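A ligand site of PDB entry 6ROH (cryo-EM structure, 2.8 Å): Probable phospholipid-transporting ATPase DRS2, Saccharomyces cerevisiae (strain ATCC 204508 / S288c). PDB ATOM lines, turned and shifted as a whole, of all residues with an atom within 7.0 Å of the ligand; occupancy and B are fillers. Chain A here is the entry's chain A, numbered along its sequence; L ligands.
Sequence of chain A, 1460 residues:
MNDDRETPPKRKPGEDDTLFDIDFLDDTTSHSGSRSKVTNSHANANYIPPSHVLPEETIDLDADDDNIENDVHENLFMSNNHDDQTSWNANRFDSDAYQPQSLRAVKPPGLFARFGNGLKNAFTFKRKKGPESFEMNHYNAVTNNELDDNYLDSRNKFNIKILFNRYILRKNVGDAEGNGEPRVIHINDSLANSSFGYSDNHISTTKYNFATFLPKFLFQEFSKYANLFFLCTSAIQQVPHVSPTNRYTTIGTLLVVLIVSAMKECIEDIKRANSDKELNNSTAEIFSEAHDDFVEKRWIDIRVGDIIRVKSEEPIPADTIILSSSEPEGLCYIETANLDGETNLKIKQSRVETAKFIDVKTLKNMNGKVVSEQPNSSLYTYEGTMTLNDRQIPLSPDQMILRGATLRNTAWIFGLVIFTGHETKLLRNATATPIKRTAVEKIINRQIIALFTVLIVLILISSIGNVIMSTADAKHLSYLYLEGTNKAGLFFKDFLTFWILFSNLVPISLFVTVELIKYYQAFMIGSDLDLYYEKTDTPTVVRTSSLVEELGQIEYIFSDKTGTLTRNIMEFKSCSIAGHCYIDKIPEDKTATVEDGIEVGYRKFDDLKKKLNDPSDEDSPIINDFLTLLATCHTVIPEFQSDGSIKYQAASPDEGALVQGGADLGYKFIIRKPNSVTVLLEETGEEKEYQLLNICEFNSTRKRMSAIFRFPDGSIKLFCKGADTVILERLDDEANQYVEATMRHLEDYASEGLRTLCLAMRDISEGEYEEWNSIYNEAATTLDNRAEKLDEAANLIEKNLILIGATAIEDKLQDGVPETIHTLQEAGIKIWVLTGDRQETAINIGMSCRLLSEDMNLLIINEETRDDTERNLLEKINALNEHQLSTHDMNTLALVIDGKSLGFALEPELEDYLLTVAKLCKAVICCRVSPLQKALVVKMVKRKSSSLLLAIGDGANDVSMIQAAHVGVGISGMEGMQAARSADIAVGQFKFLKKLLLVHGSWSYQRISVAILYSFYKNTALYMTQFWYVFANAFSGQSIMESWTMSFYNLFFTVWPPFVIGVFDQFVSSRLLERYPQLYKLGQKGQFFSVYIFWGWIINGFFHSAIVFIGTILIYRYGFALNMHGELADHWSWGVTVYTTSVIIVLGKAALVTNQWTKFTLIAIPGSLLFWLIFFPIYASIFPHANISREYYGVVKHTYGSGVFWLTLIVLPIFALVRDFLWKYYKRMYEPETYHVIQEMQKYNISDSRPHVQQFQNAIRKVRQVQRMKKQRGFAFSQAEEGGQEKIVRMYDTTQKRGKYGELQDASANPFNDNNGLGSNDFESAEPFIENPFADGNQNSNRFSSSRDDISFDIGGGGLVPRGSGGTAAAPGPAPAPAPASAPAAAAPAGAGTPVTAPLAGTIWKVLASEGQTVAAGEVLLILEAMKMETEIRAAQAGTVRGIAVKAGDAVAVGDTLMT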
ATOM      1  N   ILE A1093     -37.366  -9.548 -17.728  1.00  0.00           N
ATOM      2  CA  ILE A1093     -36.207  -9.090 -18.480  1.00  0.00           C
ATOM      3  C   ILE A1093     -35.599  -7.839 -17.860  1.00  0.00           C
ATOM      4  O   ILE A1093     -34.462  -7.474 -18.183  1.00  0.00           O
ATOM      5  CB  ILE A1093     -36.564  -8.879 -19.962  1.00  0.00           C
ATOM      6  CG1 ILE A1093     -35.356  -9.146 -20.854  1.00  0.00           C
ATOM      7  CG2 ILE A1093     -37.133  -7.487 -20.205  1.00  0.00           C
ATOM      8  CD1 ILE A1093     -35.675  -9.183 -22.325  1.00  0.00           C
ATOM      9  N   TRP A1095     -34.796  -7.880 -14.763  1.00  0.00           N
ATOM     10  CA  TRP A1095     -33.817  -8.442 -13.844  1.00  0.00           C
ATOM     11  C   TRP A1095     -32.514  -8.815 -14.525  1.00  0.00           C
ATOM     12  O   TRP A1095     -31.513  -9.005 -13.836  1.00  0.00           O
ATOM     13  CB  TRP A1095     -34.375  -9.673 -13.144  1.00  0.00           C
ATOM     14  CG  TRP A1095     -35.417  -9.357 -12.137  1.00  0.00           C
ATOM     15  CD1 TRP A1095     -36.729  -9.723 -12.178  1.00  0.00           C
ATOM     16  CD2 TRP A1095     -35.241  -8.612 -10.926  1.00  0.00           C
ATOM     17  NE1 TRP A1095     -37.380  -9.252 -11.070  1.00  0.00           N
ATOM     18  CE2 TRP A1095     -36.486  -8.562 -10.288  1.00  0.00           C
ATOM     19  CE3 TRP A1095     -34.147  -7.990 -10.323  1.00  0.00           C
ATOM     20  CZ2 TRP A1095     -36.669  -7.912  -9.079  1.00  0.00           C
ATOM     21  CZ3 TRP A1095     -34.333  -7.345  -9.130  1.00  0.00           C
ATOM     22  CH2 TRP A1095     -35.587  -7.308  -8.518  1.00  0.00           C
ATOM     23  N   GLY A1096     -32.485  -8.928 -15.847  1.00  0.00           N
ATOM     24  CA  GLY A1096     -31.227  -9.179 -16.515  1.00  0.00           C
ATOM     25  C   GLY A1096     -30.390  -7.939 -16.693  1.00  0.00           C
ATOM     26  O   GLY A1096     -29.208  -8.050 -17.050  1.00  0.00           O
ATOM     27  N   TRP A1097     -30.953  -6.764 -16.458  1.00  0.00           N
ATOM     28  CA  TRP A1097     -30.219  -5.508 -16.511  1.00  0.00           C
ATOM     29  C   TRP A1097     -29.774  -5.040 -15.132  1.00  0.00           C
ATOM     30  O   TRP A1097     -28.688  -4.481 -15.000  1.00  0.00           O
ATOM     31  CB  TRP A1097     -31.073  -4.428 -17.177  1.00  0.00           C
ATOM     32  CG  TRP A1097     -31.288  -4.646 -18.642  1.00  0.00           C
ATOM     33  CD1 TRP A1097     -32.158  -5.530 -19.208  1.00  0.00           C
ATOM     34  CD2 TRP A1097     -30.618  -3.989 -19.715  1.00  0.00           C
ATOM     35  NE1 TRP A1097     -32.074  -5.455 -20.573  1.00  0.00           N
ATOM     36  CE2 TRP A1097     -31.135  -4.516 -20.911  1.00  0.00           C
ATOM     37  CE3 TRP A1097     -29.641  -2.994 -19.795  1.00  0.00           C
ATOM     38  CZ2 TRP A1097     -30.711  -4.089 -22.163  1.00  0.00           C
ATOM     39  CZ3 TRP A1097     -29.215  -2.571 -21.034  1.00  0.00           C
ATOM     40  CH2 TRP A1097     -29.754  -3.120 -22.202  1.00  0.00           C
ATOM     41  N   ILE A1099     -29.146  -7.124 -12.550  1.00  0.00           N
ATOM     42  CA  ILE A1099     -28.027  -8.008 -12.225  1.00  0.00           C
ATOM     43  C   ILE A1099     -26.803  -7.671 -13.079  1.00  0.00           C
ATOM     44  O   ILE A1099     -25.678  -7.797 -12.612  1.00  0.00           O
ATOM     45  CB  ILE A1099     -28.481  -9.470 -12.370  1.00  0.00           C
ATOM     46  CG1 ILE A1099     -29.546  -9.787 -11.326  1.00  0.00           C
ATOM     47  CG2 ILE A1099     -27.354 -10.463 -12.184  1.00  0.00           C
ATOM     48  CD1 ILE A1099     -30.207 -11.120 -11.521  1.00  0.00           C
ATOM     49  N   ASN A1100     -27.019  -7.170 -14.293  1.00  0.00           N
ATOM     50  CA  ASN A1100     -25.901  -6.640 -15.072  1.00  0.00           C
ATOM     51  C   ASN A1100     -25.371  -5.343 -14.466  1.00  0.00           C
ATOM     52  O   ASN A1100     -24.205  -4.999 -14.672  1.00  0.00           O
ATOM     53  CB  ASN A1100     -26.317  -6.404 -16.510  1.00  0.00           C
ATOM     54  CG  ASN A1100     -25.155  -6.428 -17.458  1.00  0.00           C
ATOM     55  OD1 ASN A1100     -24.045  -6.807 -17.087  1.00  0.00           O
ATOM     56  ND2 ASN A1100     -25.389  -6.016 -18.693  1.00  0.00           N
ATOM     57  N   GLY A1101     -26.210  -4.609 -13.747  1.00  0.00           N
ATOM     58  CA  GLY A1101     -25.736  -3.442 -13.024  1.00  0.00           C
ATOM     59  C   GLY A1101     -24.965  -3.790 -11.773  1.00  0.00           C
ATOM     60  O   GLY A1101     -24.066  -3.057 -11.374  1.00  0.00           O
ATOM     61  N   PHE A1102     -25.299  -4.924 -11.144  1.00  0.00           N
ATOM     62  CA  PHE A1102     -24.547  -5.372  -9.971  1.00  0.00           C
ATOM     63  C   PHE A1102     -23.181  -5.905 -10.355  1.00  0.00           C
ATOM     64  O   PHE A1102     -22.206  -5.669  -9.637  1.00  0.00           O
ATOM     65  CB  PHE A1102     -25.320  -6.473  -9.235  1.00  0.00           C
ATOM     66  CG  PHE A1102     -26.537  -5.999  -8.504  1.00  0.00           C
ATOM     67  CD1 PHE A1102     -26.773  -4.658  -8.289  1.00  0.00           C
ATOM     68  CD2 PHE A1102     -27.454  -6.924  -8.028  1.00  0.00           C
ATOM     69  CE1 PHE A1102     -27.899  -4.248  -7.606  1.00  0.00           C
ATOM     70  CE2 PHE A1102     -28.580  -6.505  -7.342  1.00  0.00           C
ATOM     71  CZ  PHE A1102     -28.797  -5.169  -7.141  1.00  0.00           C
ATOM     72  N   PHE A1103     -23.099  -6.624 -11.470  1.00  0.00           N
ATOM     73  CA  PHE A1103     -21.844  -7.216 -11.907  1.00  0.00           C
ATOM     74  C   PHE A1103     -20.876  -6.165 -12.401  1.00  0.00           C
ATOM     75  O   PHE A1103     -19.660  -6.305 -12.210  1.00  0.00           O
ATOM     76  CB  PHE A1103     -22.128  -8.239 -13.006  1.00  0.00           C
ATOM     77  CG  PHE A1103     -20.900  -8.751 -13.691  1.00  0.00           C
ATOM     78  CD1 PHE A1103     -20.062  -9.645 -13.070  1.00  0.00           C
ATOM     79  CD2 PHE A1103     -20.610  -8.364 -14.993  1.00  0.00           C
ATOM     80  CE1 PHE A1103     -18.944 -10.134 -13.710  1.00  0.00           C
ATOM     81  CE2 PHE A1103     -19.494  -8.838 -15.643  1.00  0.00           C
ATOM     82  CZ  PHE A1103     -18.660  -9.731 -14.997  1.00  0.00           C
ATOM     83  N   HIS A1104     -21.377  -5.102 -13.021  1.00  0.00           N
ATOM     84  CA  HIS A1104     -20.499  -4.024 -13.479  1.00  0.00           C
ATOM     85  C   HIS A1104     -20.036  -3.151 -12.333  1.00  0.00           C
ATOM     86  O   HIS A1104     -18.962  -2.564 -12.395  1.00  0.00           O
ATOM     87  CB  HIS A1104     -21.207  -3.186 -14.521  1.00  0.00           C
ATOM     88  CG  HIS A1104     -21.064  -3.719 -15.910  1.00  0.00           C
ATOM     89  ND1 HIS A1104     -21.906  -3.359 -16.936  1.00  0.00           N
ATOM     90  CD2 HIS A1104     -20.179  -4.599 -16.431  1.00  0.00           C
ATOM     91  CE1 HIS A1104     -21.535  -3.989 -18.038  1.00  0.00           C
ATOM     92  NE2 HIS A1104     -20.493  -4.742 -17.758  1.00  0.00           N
ATOM     93  N   LYS A1149     -21.574   0.418 -22.852  1.00  0.00           N
ATOM     94  CA  LYS A1149     -22.704  -0.494 -22.956  1.00  0.00           C
ATOM     95  C   LYS A1149     -23.736   0.032 -23.955  1.00  0.00           C
ATOM     96  O   LYS A1149     -24.242  -0.727 -24.777  1.00  0.00           O
ATOM     97  CB  LYS A1149     -23.338  -0.692 -21.588  1.00  0.00           C
ATOM     98  CG  LYS A1149     -24.648  -1.448 -21.609  1.00  0.00           C
ATOM     99  CD  LYS A1149     -24.425  -2.921 -21.845  1.00  0.00           C
ATOM    100  CE  LYS A1149     -25.643  -3.717 -21.425  1.00  0.00           C
ATOM    101  NZ  LYS A1149     -25.424  -5.169 -21.630  1.00  0.00           N
ATOM    102  N   LEU A1152     -22.881  -0.720 -27.427  1.00  0.00           N
ATOM    103  CA  LEU A1152     -23.170  -2.093 -27.832  1.00  0.00           C
ATOM    104  C   LEU A1152     -24.655  -2.374 -27.915  1.00  0.00           C
ATOM    105  O   LEU A1152     -25.077  -3.237 -28.677  1.00  0.00           O
ATOM    106  CB  LEU A1152     -22.532  -3.088 -26.863  1.00  0.00           C
ATOM    107  CG  LEU A1152     -21.013  -3.096 -26.776  1.00  0.00           C
ATOM    108  CD1 LEU A1152     -20.555  -4.016 -25.676  1.00  0.00           C
ATOM    109  CD2 LEU A1152     -20.412  -3.499 -28.102  1.00  0.00           C
ATOM    110  N   VAL A1153     -25.443  -1.657 -27.112  1.00  0.00           N
ATOM    111  CA  VAL A1153     -26.891  -1.805 -27.117  1.00  0.00           C
ATOM    112  C   VAL A1153     -27.499  -1.248 -28.402  1.00  0.00           C
ATOM    113  O   VAL A1153     -28.411  -1.852 -28.981  1.00  0.00           O
ATOM    114  CB  VAL A1153     -27.461  -1.145 -25.850  1.00  0.00           C
ATOM    115  CG1 VAL A1153     -28.912  -0.901 -25.966  1.00  0.00           C
ATOM    116  CG2 VAL A1153     -27.235  -2.049 -24.668  1.00  0.00           C
ATOM    117  N   ARG A1219     -17.912  -9.302 -21.394  1.00  0.00           N
ATOM    118  CA  ARG A1219     -19.016 -10.256 -21.496  1.00  0.00           C
ATOM    119  C   ARG A1219     -20.118  -9.691 -22.375  1.00  0.00           C
ATOM    120  O   ARG A1219     -20.847 -10.455 -23.025  1.00  0.00           O
ATOM    121  CB  ARG A1219     -19.530 -10.610 -20.100  1.00  0.00           C
ATOM    122  CG  ARG A1219     -20.357 -11.893 -20.008  1.00  0.00           C
ATOM    123  CD  ARG A1219     -21.836 -11.633 -20.112  1.00  0.00           C
ATOM    124  NE  ARG A1219     -22.252 -10.674 -19.097  1.00  0.00           N
ATOM    125  CZ  ARG A1219     -23.373  -9.976 -19.145  1.00  0.00           C
ATOM    126  NH1 ARG A1219     -24.215 -10.135 -20.151  1.00  0.00           N
ATOM    127  NH2 ARG A1219     -23.649  -9.125 -18.174  1.00  0.00           N
ATOM    128  N   ASP A1220     -20.265  -8.371 -22.414  1.00  0.00           N
ATOM    129  CA  ASP A1220     -21.311  -7.772 -23.238  1.00  0.00           C
ATOM    130  C   ASP A1220     -20.896  -7.714 -24.705  1.00  0.00           C
ATOM    131  O   ASP A1220     -21.747  -7.631 -25.585  1.00  0.00           O
ATOM    132  CB  ASP A1220     -21.647  -6.382 -22.726  1.00  0.00           C
ATOM    133  CG  ASP A1220     -22.200  -6.387 -21.328  1.00  0.00           C
ATOM    134  OD1 ASP A1220     -22.554  -7.471 -20.837  1.00  0.00           O
ATOM    135  OD2 ASP A1220     -22.298  -5.311 -20.724  1.00  0.00           O
ATOM    136  N   TRP A1223     -21.530 -11.577 -25.639  1.00  0.00           N
ATOM    137  CA  TRP A1223     -22.929 -11.956 -25.736  1.00  0.00           C
ATOM    138  C   TRP A1223     -23.590 -11.310 -26.947  1.00  0.00           C
ATOM    139  O   TRP A1223     -24.473 -11.909 -27.569  1.00  0.00           O
ATOM    140  CB  TRP A1223     -23.673 -11.581 -24.461  1.00  0.00           C
ATOM    141  CG  TRP A1223     -25.104 -11.983 -24.498  1.00  0.00           C
ATOM    142  CD1 TRP A1223     -26.174 -11.162 -24.734  1.00  0.00           C
ATOM    143  CD2 TRP A1223     -25.630 -13.295 -24.301  1.00  0.00           C
ATOM    144  NE1 TRP A1223     -27.336 -11.899 -24.678  1.00  0.00           N
ATOM    145  CE2 TRP A1223     -27.039 -13.199 -24.416  1.00  0.00           C
ATOM    146  CE3 TRP A1223     -25.062 -14.539 -24.026  1.00  0.00           C
ATOM    147  CZ2 TRP A1223     -27.867 -14.306 -24.283  1.00  0.00           C
ATOM    148  CZ3 TRP A1223     -25.891 -15.627 -23.886  1.00  0.00           C
ATOM    149  CH2 TRP A1223     -27.275 -15.505 -24.013  1.00  0.00           C
ATOM    150  N   LYS A1224     -23.181 -10.086 -27.292  1.00  0.00           N
ATOM    151  CA  LYS A1224     -23.730  -9.419 -28.464  1.00  0.00           C
ATOM    152  C   LYS A1224     -23.235 -10.076 -29.746  1.00  0.00           C
ATOM    153  O   LYS A1224     -23.957 -10.125 -30.751  1.00  0.00           O
ATOM    154  CB  LYS A1224     -23.357  -7.934 -28.448  1.00  0.00           C
ATOM    155  CG  LYS A1224     -23.993  -7.081 -29.522  1.00  0.00           C
ATOM    156  CD  LYS A1224     -23.035  -5.985 -29.967  1.00  0.00           C
ATOM    157  CE  LYS A1224     -23.613  -5.163 -31.101  1.00  0.00           C
ATOM    158  NZ  LYS A1224     -24.945  -4.594 -30.756  1.00  0.00           N
ATOM    159  N   LYS A1227     -25.194 -13.381 -29.866  1.00  0.00           N
ATOM    160  CA  LYS A1227     -26.595 -13.168 -30.216  1.00  0.00           C
ATOM    161  C   LYS A1227     -26.764 -12.914 -31.711  1.00  0.00           C
ATOM    162  O   LYS A1227     -27.835 -13.140 -32.261  1.00  0.00           O
ATOM    163  CB  LYS A1227     -27.157 -12.008 -29.413  1.00  0.00           C
ATOM    164  CG  LYS A1227     -28.678 -11.991 -29.290  1.00  0.00           C
ATOM    165  CD  LYS A1227     -29.187 -13.125 -28.413  1.00  0.00           C
ATOM    166  CE  LYS A1227     -30.699 -13.108 -28.322  1.00  0.00           C
ATOM    167  NZ  LYS A1227     -31.238 -14.199 -27.477  1.00  0.00           N
ATOM    168  N   GLU A1233     -33.871 -14.543 -32.850  1.00  0.00           N
ATOM    169  CA  GLU A1233     -35.300 -14.313 -32.837  1.00  0.00           C
ATOM    170  C   GLU A1233     -35.698 -13.556 -34.099  1.00  0.00           C
ATOM    171  O   GLU A1233     -34.846 -13.133 -34.895  1.00  0.00           O
ATOM    172  CB  GLU A1233     -35.738 -13.556 -31.592  1.00  0.00           C
ATOM    173  CG  GLU A1233     -35.114 -12.193 -31.425  1.00  0.00           C
ATOM    174  CD  GLU A1233     -33.844 -12.233 -30.597  1.00  0.00           C
ATOM    175  OE1 GLU A1233     -33.306 -13.339 -30.382  1.00  0.00           O
ATOM    176  OE2 GLU A1233     -33.391 -11.159 -30.148  1.00  0.00           O
ATOM    177  N   TYR A1235     -37.133 -10.649 -35.149  1.00  0.00           N
ATOM    178  CA  TYR A1235     -36.803  -9.305 -35.595  1.00  0.00           C
ATOM    179  C   TYR A1235     -35.310  -9.198 -35.912  1.00  0.00           C
ATOM    180  O   TYR A1235     -34.918  -9.210 -37.071  1.00  0.00           O
ATOM    181  CB  TYR A1235     -37.215  -8.249 -34.553  1.00  0.00           C
ATOM    182  CG  TYR A1235     -36.289  -8.057 -33.368  1.00  0.00           C
ATOM    183  CD1 TYR A1235     -36.391  -8.864 -32.247  1.00  0.00           C
ATOM    184  CD2 TYR A1235     -35.334  -7.044 -33.353  1.00  0.00           C
ATOM    185  CE1 TYR A1235     -35.557  -8.677 -31.145  1.00  0.00           C
ATOM    186  CE2 TYR A1235     -34.497  -6.849 -32.272  1.00  0.00           C
ATOM    187  CZ  TYR A1235     -34.615  -7.671 -31.168  1.00  0.00           C
ATOM    188  OH  TYR A1235     -33.786  -7.484 -30.095  1.00  0.00           O
HETATM  189  O1  LIG L   1     -28.455 -10.363 -21.682  1.00  0.00           O
HETATM  190  O2  LIG L   1     -29.106  -8.354 -23.010  1.00  0.00           O
HETATM  191  P1  LIG L   1     -27.975  -8.740 -21.858  1.00  0.00           P
HETATM  192  O3  LIG L   1     -28.259  -7.986 -20.592  1.00  0.00           O
HETATM  193  O4  LIG L   1     -26.657  -8.804 -22.539  1.00  0.00           O
HETATM  194  C1  LIG L   1     -29.101 -10.704 -20.508  1.00  0.00           C
HETATM  195  C2  LIG L   1     -28.084 -11.375 -19.551  1.00  0.00           C
HETATM  196  O5  LIG L   1     -28.096 -12.764 -19.772  1.00  0.00           O
HETATM  197  O6  LIG L   1     -26.409 -12.623 -21.246  1.00  0.00           O
HETATM  198  C3  LIG L   1     -27.040 -13.272 -20.453  1.00  0.00           C
HETATM  199  C4  LIG L   1     -28.453 -11.126 -18.074  1.00  0.00           C
HETATM  200  C5  LIG L   1     -26.471 -10.983 -16.756  1.00  0.00           C
HETATM  201  O7  LIG L   1     -26.104  -9.950 -17.282  1.00  0.00           O
HETATM  202  O8  LIG L   1     -27.464 -11.754 -17.264  1.00  0.00           O
HETATM  203  C6  LIG L   1     -25.921 -11.569 -15.485  1.00  0.00           C
HETATM  204  C7  LIG L   1     -24.766 -10.766 -14.936  1.00  0.00           C
HETATM  205  C8  LIG L   1     -26.793 -14.699 -20.082  1.00  0.00           C
HETATM  206  C9  LIG L   1     -25.321 -15.071 -20.169  1.00  0.00           C
HETATM  207  C10 LIG L   1     -24.748 -15.395 -18.794  1.00  0.00           C
HETATM  208  N1  LIG L   1     -31.340  -9.733 -25.395  1.00  0.00           N
HETATM  209  C11 LIG L   1     -30.366  -8.697 -25.032  1.00  0.00           C
HETATM  210  C12 LIG L   1     -29.420  -9.288 -23.978  1.00  0.00           C
HETATM  211  C13 LIG L   1     -29.491  -8.072 -26.149  1.00  0.00           C
HETATM  212  O9  LIG L   1     -28.496  -7.363 -25.792  1.00  0.00           O
HETATM  213  O10 LIG L   1     -29.815  -8.294 -27.318  1.00  0.00           O
HETATM  214  C14 LIG L   1     -23.441 -11.276 -15.472  1.00  0.00           C
HETATM  215  C15 LIG L   1     -22.833 -12.297 -14.522  1.00  0.00           C
HETATM  216  C16 LIG L   1     -21.451 -12.730 -14.973  1.00  0.00           C
HETATM  217  C17 LIG L   1     -23.285 -15.807 -18.918  1.00  0.00           C
HETATM  218  C18 LIG L   1     -22.659 -16.021 -17.551  1.00  0.00           C
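O of Gly 1096 touches C4 of the ligand (3.3 Å). Ile 1099 touches the ligand (CG2 to C6, 3.8 Å). Asn 1100 touches the ligand. Phe 1103 touches the ligand. Trp 1223 touches the ligand (CD2 to O6, 3.2 Å). Hydrophobic or aromatic side chains that line the ligand: Ile 1099, Phe 1103 and Trp 1223.
The guanidinium group of Arg 1219 sits at hydrogen-bond distance from the side-chain amide oxygen of Asn 1100, 2.6 Å away. NH1 of Arg 1219 is in salt-bridge range of OD1 of Asp 1220 (3.2 Å). The side-chain amino group (NZ) of Lys 1149 lies close to the side-chain amide nitrogen (ND2) of Asn 1100, 3.1 Å away. OD2 of Asp 1220 lies within salt-bridge range of NZ of Lys 1149.
The guanidinium group (NH1) of Arg 1219 is in salt-bridge range of an oxygen (O4) of the ligand (3.7 Å). NZ of Lys 1149 is in salt-bridge range of O4 of the ligand, 3.9 Å away.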
